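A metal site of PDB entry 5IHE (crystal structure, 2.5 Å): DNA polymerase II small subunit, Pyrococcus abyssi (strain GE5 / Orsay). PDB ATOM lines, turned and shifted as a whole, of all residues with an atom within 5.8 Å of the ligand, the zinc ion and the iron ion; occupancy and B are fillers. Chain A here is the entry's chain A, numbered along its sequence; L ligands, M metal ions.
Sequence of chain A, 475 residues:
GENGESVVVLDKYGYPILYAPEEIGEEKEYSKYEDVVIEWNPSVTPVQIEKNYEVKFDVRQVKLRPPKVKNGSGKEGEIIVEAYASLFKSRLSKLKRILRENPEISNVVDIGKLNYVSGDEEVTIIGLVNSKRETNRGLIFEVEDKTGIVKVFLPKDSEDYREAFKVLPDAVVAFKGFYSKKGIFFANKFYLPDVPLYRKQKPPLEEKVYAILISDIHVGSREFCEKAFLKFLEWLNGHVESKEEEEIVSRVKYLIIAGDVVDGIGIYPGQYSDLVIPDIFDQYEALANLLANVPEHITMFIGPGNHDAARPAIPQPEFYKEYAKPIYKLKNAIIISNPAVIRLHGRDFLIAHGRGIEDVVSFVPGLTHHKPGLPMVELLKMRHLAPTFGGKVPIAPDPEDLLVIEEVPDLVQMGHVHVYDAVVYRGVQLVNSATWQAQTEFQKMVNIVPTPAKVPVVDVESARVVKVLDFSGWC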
ATOM      1  N   ASP A 216      10.768 -10.880 -11.884  1.00  0.00           N
ATOM      2  CA  ASP A 216       9.637  -9.967 -12.020  1.00  0.00           C
ATOM      3  C   ASP A 216       9.696  -8.825 -11.019  1.00  0.00           C
ATOM      4  O   ASP A 216       8.781  -8.627 -10.206  1.00  0.00           O
ATOM      5  CB  ASP A 216       8.320 -10.745 -11.989  1.00  0.00           C
ATOM      6  CG  ASP A 216       8.234 -11.772 -13.087  1.00  0.00           C
ATOM      7  OD1 ASP A 216       7.596 -11.478 -14.122  1.00  0.00           O
ATOM      8  OD2 ASP A 216       8.846 -12.855 -12.941  1.00  0.00           O
ATOM      9  N   HIS A 218       9.886  -5.592 -11.925  1.00  0.00           N
ATOM     10  CA  HIS A 218       8.989  -4.609 -12.528  1.00  0.00           C
ATOM     11  C   HIS A 218       9.252  -3.180 -12.068  1.00  0.00           C
ATOM     12  O   HIS A 218       8.310  -2.453 -11.752  1.00  0.00           O
ATOM     13  CB  HIS A 218       7.504  -5.006 -12.335  1.00  0.00           C
ATOM     14  CG  HIS A 218       7.086  -6.156 -13.177  1.00  0.00           C
ATOM     15  ND1 HIS A 218       6.609  -5.978 -14.451  1.00  0.00           N
ATOM     16  CD2 HIS A 218       7.148  -7.481 -12.916  1.00  0.00           C
ATOM     17  CE1 HIS A 218       6.366  -7.189 -14.928  1.00  0.00           C
ATOM     18  NE2 HIS A 218       6.687  -8.127 -14.043  1.00  0.00           N
ATOM     19  N   GLY A 259      13.993 -12.514 -15.523  1.00  0.00           N
ATOM     20  CA  GLY A 259      13.107 -11.673 -16.320  1.00  0.00           C
ATOM     21  C   GLY A 259      12.195 -10.687 -15.638  1.00  0.00           C
ATOM     22  O   GLY A 259      11.982 -10.743 -14.426  1.00  0.00           O
ATOM     23  N   ASP A 260      11.602  -9.777 -16.476  1.00  0.00           N
ATOM     24  CA  ASP A 260      10.730  -8.647 -16.154  1.00  0.00           C
ATOM     25  C   ASP A 260      11.349  -7.774 -15.054  1.00  0.00           C
ATOM     26  O   ASP A 260      10.721  -7.462 -14.045  1.00  0.00           O
ATOM     27  CB  ASP A 260       9.300  -9.095 -15.853  1.00  0.00           C
ATOM     28  CG  ASP A 260       8.538  -9.592 -17.059  1.00  0.00           C
ATOM     29  OD1 ASP A 260       8.934  -9.283 -18.179  1.00  0.00           O
ATOM     30  OD2 ASP A 260       7.550 -10.316 -16.879  1.00  0.00           O
ATOM     31  N   ILE A 267       3.579  -2.181 -23.091  1.00  0.00           N
ATOM     32  CA  ILE A 267       3.403  -3.649 -22.977  1.00  0.00           C
ATOM     33  C   ILE A 267       1.920  -4.035 -23.143  1.00  0.00           C
ATOM     34  O   ILE A 267       1.604  -5.016 -23.829  1.00  0.00           O
ATOM     35  CB  ILE A 267       4.070  -4.205 -21.677  1.00  0.00           C
ATOM     36  CG1 ILE A 267       5.569  -3.804 -21.571  1.00  0.00           C
ATOM     37  CG2 ILE A 267       3.888  -5.718 -21.521  1.00  0.00           C
ATOM     38  CD1 ILE A 267       6.509  -4.182 -22.772  1.00  0.00           C
ATOM     39  N   GLY A 305      12.823 -10.709 -19.726  1.00  0.00           N
ATOM     40  CA  GLY A 305      11.432 -11.162 -19.691  1.00  0.00           C
ATOM     41  C   GLY A 305      10.647 -10.491 -20.808  1.00  0.00           C
ATOM     42  O   GLY A 305      11.244  -9.817 -21.647  1.00  0.00           O
ATOM     43  N   ASN A 306       9.311 -10.617 -20.822  1.00  0.00           N
ATOM     44  CA  ASN A 306       8.487 -10.007 -21.877  1.00  0.00           C
ATOM     45  C   ASN A 306       8.209  -8.492 -21.712  1.00  0.00           C
ATOM     46  O   ASN A 306       7.734  -7.870 -22.655  1.00  0.00           O
ATOM     47  CB  ASN A 306       7.167 -10.778 -22.074  1.00  0.00           C
ATOM     48  CG  ASN A 306       6.348 -10.926 -20.824  1.00  0.00           C
ATOM     49  OD1 ASN A 306       6.755 -11.576 -19.861  1.00  0.00           O
ATOM     50  ND2 ASN A 306       5.157 -10.339 -20.827  1.00  0.00           N
ATOM     51  N   HIS A 307       8.513  -7.912 -20.545  1.00  0.00           N
ATOM     52  CA  HIS A 307       8.319  -6.472 -20.283  1.00  0.00           C
ATOM     53  C   HIS A 307       9.586  -5.715 -20.605  1.00  0.00           C
ATOM     54  O   HIS A 307       9.557  -4.505 -20.819  1.00  0.00           O
ATOM     55  CB  HIS A 307       7.931  -6.221 -18.813  1.00  0.00           C
ATOM     56  CG  HIS A 307       6.482  -6.495 -18.506  1.00  0.00           C
ATOM     57  ND1 HIS A 307       5.652  -5.496 -18.048  1.00  0.00           N
ATOM     58  CD2 HIS A 307       5.780  -7.639 -18.619  1.00  0.00           C
ATOM     59  CE1 HIS A 307       4.462  -6.060 -17.887  1.00  0.00           C
ATOM     60  NE2 HIS A 307       4.489  -7.343 -18.213  1.00  0.00           N
ATOM     61  N   HIS A 353      12.205 -17.365 -18.510  1.00  0.00           N
ATOM     62  CA  HIS A 353      11.260 -16.409 -17.951  1.00  0.00           C
ATOM     63  C   HIS A 353       9.969 -17.059 -17.499  1.00  0.00           C
ATOM     64  O   HIS A 353       9.458 -16.708 -16.445  1.00  0.00           O
ATOM     65  CB  HIS A 353      11.003 -15.212 -18.858  1.00  0.00           C
ATOM     66  CG  HIS A 353      10.119 -14.186 -18.218  1.00  0.00           C
ATOM     67  ND1 HIS A 353      10.420 -13.645 -16.980  1.00  0.00           N
ATOM     68  CD2 HIS A 353       8.945 -13.675 -18.637  1.00  0.00           C
ATOM     69  CE1 HIS A 353       9.433 -12.831 -16.685  1.00  0.00           C
ATOM     70  NE2 HIS A 353       8.515 -12.819 -17.651  1.00  0.00           N
ATOM     71  N   ARG A 355       7.217 -18.153 -19.976  1.00  0.00           N
ATOM     72  CA  ARG A 355       6.147 -17.976 -20.951  1.00  0.00           C
ATOM     73  C   ARG A 355       5.354 -19.254 -21.194  1.00  0.00           C
ATOM     74  O   ARG A 355       4.133 -19.194 -21.392  1.00  0.00           O
ATOM     75  CB  ARG A 355       6.670 -17.373 -22.277  1.00  0.00           C
ATOM     76  CG  ARG A 355       7.273 -15.956 -22.189  1.00  0.00           C
ATOM     77  CD  ARG A 355       6.377 -14.850 -21.606  1.00  0.00           C
ATOM     78  NE  ARG A 355       5.057 -14.750 -22.245  1.00  0.00           N
ATOM     79  CZ  ARG A 355       4.800 -14.042 -23.352  1.00  0.00           C
ATOM     80  NH1 ARG A 355       5.770 -13.365 -23.959  1.00  0.00           N
ATOM     81  NH2 ARG A 355       3.578 -14.022 -23.847  1.00  0.00           N
ATOM     82  N   GLU A 358       2.075 -20.307 -19.053  1.00  0.00           N
ATOM     83  CA  GLU A 358       0.803 -19.796 -19.585  1.00  0.00           C
ATOM     84  C   GLU A 358       0.204 -20.760 -20.586  1.00  0.00           C
ATOM     85  O   GLU A 358      -0.999 -20.980 -20.545  1.00  0.00           O
ATOM     86  CB  GLU A 358       0.978 -18.430 -20.247  1.00  0.00           C
ATOM     87  CG  GLU A 358       0.776 -17.284 -19.271  1.00  0.00           C
ATOM     88  CD  GLU A 358       0.524 -15.908 -19.846  1.00  0.00           C
ATOM     89  OE1 GLU A 358       1.307 -15.475 -20.711  1.00  0.00           O
ATOM     90  OE2 GLU A 358      -0.607 -15.405 -19.628  1.00  0.00           O
ATOM     91  N   HIS A 369      -2.528 -21.338 -12.211  1.00  0.00           N
ATOM     92  CA  HIS A 369      -1.572 -20.596 -11.381  1.00  0.00           C
ATOM     93  C   HIS A 369      -2.018 -20.852  -9.914  1.00  0.00           C
ATOM     94  O   HIS A 369      -2.836 -21.752  -9.694  1.00  0.00           O
ATOM     95  CB  HIS A 369      -1.430 -19.104 -11.803  1.00  0.00           C
ATOM     96  CG  HIS A 369      -2.457 -18.152 -11.272  1.00  0.00           C
ATOM     97  ND1 HIS A 369      -2.081 -16.998 -10.581  1.00  0.00           N
ATOM     98  CD2 HIS A 369      -3.806 -18.164 -11.381  1.00  0.00           C
ATOM     99  CE1 HIS A 369      -3.211 -16.372 -10.265  1.00  0.00           C
ATOM    100  NE2 HIS A 369      -4.269 -17.036 -10.727  1.00  0.00           N
ATOM    101  N   LYS A 392       0.068 -15.284 -26.827  1.00  0.00           N
ATOM    102  CA  LYS A 392       0.707 -13.966 -26.752  1.00  0.00           C
ATOM    103  C   LYS A 392       2.222 -14.254 -26.737  1.00  0.00           C
ATOM    104  O   LYS A 392       3.017 -13.330 -26.896  1.00  0.00           O
ATOM    105  CB  LYS A 392       0.273 -13.181 -25.497  1.00  0.00           C
ATOM    106  CG  LYS A 392      -1.194 -12.743 -25.487  1.00  0.00           C
ATOM    107  CD  LYS A 392      -2.058 -13.696 -24.661  1.00  0.00           C
ATOM    108  CE  LYS A 392      -3.301 -13.045 -24.103  1.00  0.00           C
ATOM    109  NZ  LYS A 392      -4.103 -14.005 -23.309  1.00  0.00           N
ATOM    110  N   HIS A 416       7.681 -14.974 -14.504  1.00  0.00           N
ATOM    111  CA  HIS A 416       6.520 -14.631 -15.330  1.00  0.00           C
ATOM    112  C   HIS A 416       5.159 -14.704 -14.627  1.00  0.00           C
ATOM    113  O   HIS A 416       4.434 -13.729 -14.742  1.00  0.00           O
ATOM    114  CB  HIS A 416       6.491 -15.450 -16.643  1.00  0.00           C
ATOM    115  CG  HIS A 416       5.404 -15.059 -17.584  1.00  0.00           C
ATOM    116  ND1 HIS A 416       5.330 -13.784 -18.114  1.00  0.00           N
ATOM    117  CD2 HIS A 416       4.378 -15.788 -18.073  1.00  0.00           C
ATOM    118  CE1 HIS A 416       4.258 -13.772 -18.897  1.00  0.00           C
ATOM    119  NE2 HIS A 416       3.660 -14.957 -18.899  1.00  0.00           N
ATOM    120  N   VAL A 417       4.762 -15.824 -13.978  1.00  0.00           N
ATOM    121  CA  VAL A 417       3.400 -15.957 -13.425  1.00  0.00           C
ATOM    122  C   VAL A 417       3.135 -15.179 -12.101  1.00  0.00           C
ATOM    123  O   VAL A 417       1.954 -15.030 -11.730  1.00  0.00           O
ATOM    124  CB  VAL A 417       2.922 -17.425 -13.297  1.00  0.00           C
ATOM    125  CG1 VAL A 417       3.000 -18.125 -14.646  1.00  0.00           C
ATOM    126  CG2 VAL A 417       3.692 -18.189 -12.234  1.00  0.00           C
ATOM    127  N   HIS A 418       4.188 -14.691 -11.430  1.00  0.00           N
ATOM    128  CA  HIS A 418       4.123 -13.866 -10.201  1.00  0.00           C
ATOM    129  C   HIS A 418       3.644 -14.627  -8.952  1.00  0.00           C
ATOM    130  O   HIS A 418       3.315 -13.992  -7.943  1.00  0.00           O
ATOM    131  CB  HIS A 418       3.262 -12.601 -10.433  1.00  0.00           C
ATOM    132  CG  HIS A 418       3.891 -11.594 -11.356  1.00  0.00           C
ATOM    133  ND1 HIS A 418       3.477 -10.281 -11.363  1.00  0.00           N
ATOM    134  CD2 HIS A 418       4.884 -11.737 -12.253  1.00  0.00           C
ATOM    135  CE1 HIS A 418       4.223  -9.663 -12.253  1.00  0.00           C
ATOM    136  NE2 HIS A 418       5.085 -10.503 -12.817  1.00  0.00           N
ATOM    137  N   THR A 435       7.566 -12.564  -7.681  1.00  0.00           N
ATOM    138  CA  THR A 435       7.627 -11.170  -8.145  1.00  0.00           C
ATOM    139  C   THR A 435       7.905 -10.174  -7.002  1.00  0.00           C
ATOM    140  O   THR A 435       7.751 -10.509  -5.826  1.00  0.00           O
ATOM    141  CB  THR A 435       6.265 -10.804  -8.816  1.00  0.00           C
ATOM    142  OG1 THR A 435       6.339  -9.533  -9.436  1.00  0.00           O
ATOM    143  CG2 THR A 435       5.073 -10.846  -7.845  1.00  0.00           C
ATOM    144  N   GLN A 437       6.313  -7.202  -7.522  1.00  0.00           N
ATOM    145  CA  GLN A 437       5.195  -6.363  -7.952  1.00  0.00           C
ATOM    146  C   GLN A 437       3.891  -6.825  -7.335  1.00  0.00           C
ATOM    147  O   GLN A 437       3.494  -7.965  -7.531  1.00  0.00           O
ATOM    148  CB  GLN A 437       5.104  -6.358  -9.491  1.00  0.00           C
ATOM    149  CG  GLN A 437       3.938  -5.526 -10.031  1.00  0.00           C
ATOM    150  CD  GLN A 437       3.799  -5.502 -11.529  1.00  0.00           C
ATOM    151  OE1 GLN A 437       3.599  -6.538 -12.186  1.00  0.00           O
ATOM    152  NE2 GLN A 437       3.827  -4.323 -12.084  1.00  0.00           N
ATOM    153  N   PHE A 442      -4.682  -4.091 -14.097  1.00  0.00           N
ATOM    154  CA  PHE A 442      -4.790  -5.071 -15.178  1.00  0.00           C
ATOM    155  C   PHE A 442      -4.829  -6.506 -14.677  1.00  0.00           C
ATOM    156  O   PHE A 442      -5.647  -7.285 -15.181  1.00  0.00           O
ATOM    157  CB  PHE A 442      -3.680  -4.866 -16.210  1.00  0.00           C
ATOM    158  CG  PHE A 442      -3.968  -5.496 -17.543  1.00  0.00           C
ATOM    159  CD1 PHE A 442      -3.448  -6.747 -17.868  1.00  0.00           C
ATOM    160  CD2 PHE A 442      -4.788  -4.861 -18.470  1.00  0.00           C
ATOM    161  CE1 PHE A 442      -3.737  -7.345 -19.095  1.00  0.00           C
ATOM    162  CE2 PHE A 442      -5.053  -5.455 -19.714  1.00  0.00           C
ATOM    163  CZ  PHE A 442      -4.523  -6.694 -20.005  1.00  0.00           C
ATOM    164  N   GLN A 443      -3.955  -6.864 -13.698  1.00  0.00           N
ATOM    165  CA  GLN A 443      -3.888  -8.194 -13.072  1.00  0.00           C
ATOM    166  C   GLN A 443      -5.229  -8.533 -12.389  1.00  0.00           C
ATOM    167  O   GLN A 443      -5.734  -9.630 -12.573  1.00  0.00           O
ATOM    168  CB  GLN A 443      -2.710  -8.292 -12.087  1.00  0.00           C
ATOM    169  CG  GLN A 443      -1.328  -8.421 -12.767  1.00  0.00           C
ATOM    170  CD  GLN A 443      -0.135  -8.064 -11.884  1.00  0.00           C
ATOM    171  OE1 GLN A 443      -0.233  -7.800 -10.690  1.00  0.00           O
ATOM    172  NE2 GLN A 443       1.050  -8.055 -12.463  1.00  0.00           N
ATOM    173  N   VAL A 446      -7.803  -9.496 -15.091  1.00  0.00           N
ATOM    174  CA  VAL A 446      -7.548 -10.799 -15.714  1.00  0.00           C
ATOM    175  C   VAL A 446      -7.421 -11.921 -14.642  1.00  0.00           C
ATOM    176  O   VAL A 446      -7.009 -13.049 -14.948  1.00  0.00           O
ATOM    177  CB  VAL A 446      -6.370 -10.780 -16.740  1.00  0.00           C
ATOM    178  CG1 VAL A 446      -6.665  -9.842 -17.902  1.00  0.00           C
ATOM    179  CG2 VAL A 446      -5.032 -10.436 -16.074  1.00  0.00           C
ATOM    180  N   ILE A 448      -5.358 -12.317 -11.914  1.00  0.00           N
ATOM    181  CA  ILE A 448      -4.025 -12.762 -11.497  1.00  0.00           C
ATOM    182  C   ILE A 448      -3.766 -12.246 -10.075  1.00  0.00           C
ATOM    183  O   ILE A 448      -3.824 -11.028  -9.835  1.00  0.00           O
ATOM    184  CB  ILE A 448      -2.890 -12.408 -12.532  1.00  0.00           C
ATOM    185  CG1 ILE A 448      -2.704 -13.532 -13.593  1.00  0.00           C
ATOM    186  CG2 ILE A 448      -1.520 -12.150 -11.848  1.00  0.00           C
ATOM    187  CD1 ILE A 448      -3.679 -13.585 -14.711  1.00  0.00           C
HETATM  188  O1  LIG L   1       2.669 -11.595 -16.182  1.00  0.00           O
HETATM  189  C1  LIG L   1       2.122 -11.765 -14.843  1.00  0.00           C
HETATM  190  C2  LIG L   1       0.920 -12.696 -14.888  1.00  0.00           C
HETATM  191  O2  LIG L   1      -0.110 -12.114 -15.700  1.00  0.00           O
HETATM  192  C3  LIG L   1       1.148 -14.107 -15.430  1.00  0.00           C
HETATM  193  O3  LIG L   1       0.433 -15.069 -14.648  1.00  0.00           O
HETATM  194  C4  LIG L   1       0.597 -14.034 -16.848  1.00  0.00           C
HETATM  195  C5  LIG L   1      -0.531 -13.041 -16.696  1.00  0.00           C
HETATM  196  N1  LIG L   1      -0.895 -12.286 -17.898  1.00  0.00           N
HETATM  197  C6  LIG L   1      -0.114 -11.359 -18.546  1.00  0.00           C
HETATM  198  N2  LIG L   1      -0.727 -10.740 -19.525  1.00  0.00           N
HETATM  199  C7  LIG L   1      -1.993 -11.318 -19.532  1.00  0.00           C
HETATM  200  C8  LIG L   1      -3.123 -11.085 -20.332  1.00  0.00           C
HETATM  201  N3  LIG L   1      -3.156 -10.212 -21.340  1.00  0.00           N
HETATM  202  N4  LIG L   1      -4.239 -11.811 -20.063  1.00  0.00           N
HETATM  203  C9  LIG L   1      -4.204 -12.707 -19.070  1.00  0.00           C
HETATM  204  N5  LIG L   1      -3.184 -13.018 -18.257  1.00  0.00           N
HETATM  205  C10 LIG L   1      -2.103 -12.281 -18.535  1.00  0.00           C
HETATM  206  P1  LIG L   1       3.481 -10.302 -16.709  1.00  0.00           P
HETATM  207  O4  LIG L   1       4.908 -10.493 -16.226  1.00  0.00           O
HETATM  208  O5  LIG L   1       2.960  -9.045 -15.988  1.00  0.00           O
HETATM  209  O6  LIG L   1       3.250 -10.208 -18.209  1.00  0.00           O
HETATM  210 ZN    ZN M   1       6.431 -11.858 -17.757  1.00  0.00          ZN
HETATM  211 FE    FE M   2       6.256 -10.209 -14.696  1.00  0.00          FE
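OE2 of Glu 358 touches C4 of the ligand (3.3 Å).
Lys 392 touches the ligand (NZ to N4, 3.9 Å).
CE1 of Phe 442 touches N3 of the ligand, 3.7 Å away.
CB of Val 446 touches C9 of the ligand (3.7 Å).
CD1 of Ile 448 touches N5 of the ligand, 3.6 Å away.
Of the 22 residues printed, 13 come within 4 Å of the ligand.
An oxygen (O6) of the ligand sits at hydrogen-bond distance from a ring nitrogen (NE2) of His 307 (3.1 Å).
The backbone carbonyl oxygen (O) of Val 417 is in hydrogen-bond range of an oxygen (O3) of the ligand.
The iron ion is bound by the side-chain carboxylate (OD1) of Asp 216 (1.9 Å), an oxygen (O4) of the ligand (2.1 Å), a ring nitrogen (NE2) of His 218 (2.2 Å), a ring nitrogen (NE2) of His 418 (2.2 Å) and the side-chain carboxylate (OD2) of Asp 260 (2.5 Å).
The iron ion has five donor atoms within binding distance.
Of the 22 residues printed, 5 come within 4 Å of the iron ion.
Along chain A the residues within 4 Å of the iron ion span positions 216 to 418.
OD2 of Asp 260 binds the zinc ion (2.1 Å).
The zinc ion is bound by OD1 of Asn 306, at 2.1 Å.
ND1 of His 416 binds the zinc ion (2.2 Å).
NE2 of His 353 is bound to the zinc ion.
O4 of the ligand is bound to the zinc ion, 2.6 Å away.
The zinc ion has five donor atoms within binding distance.
The backbone NH (N) of His 416 lies within hydrogen-bond range of the side-chain carboxylate (OD2) of Asp 216 (2.9 Å).
O of Asp 216 is in hydrogen-bond range of OG1 of Thr 435.
The backbone carbonyl oxygen (O) of Gly 259 sits at hydrogen-bond distance from the backbone NH (N) of Asp 216 (2.8 Å).
OD1 of Asp 260 sits at hydrogen-bond distance from N of His 307, at 2.8 Å.
ND1 of His 418 is in hydrogen-bond range of NE2 of Gln 443, 3.5 Å away.
NE2 of His 416 lies within hydrogen-bond range of OE1 of Glu 358 (3.0 Å).
The backbone NH (N) of Ile 448 sits at hydrogen-bond distance from the backbone carbonyl oxygen (O) of Gln 443, at 2.8 Å.
O of Lys 392 lies within hydrogen-bond range of NH2 of Arg 355 (3.2 Å).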
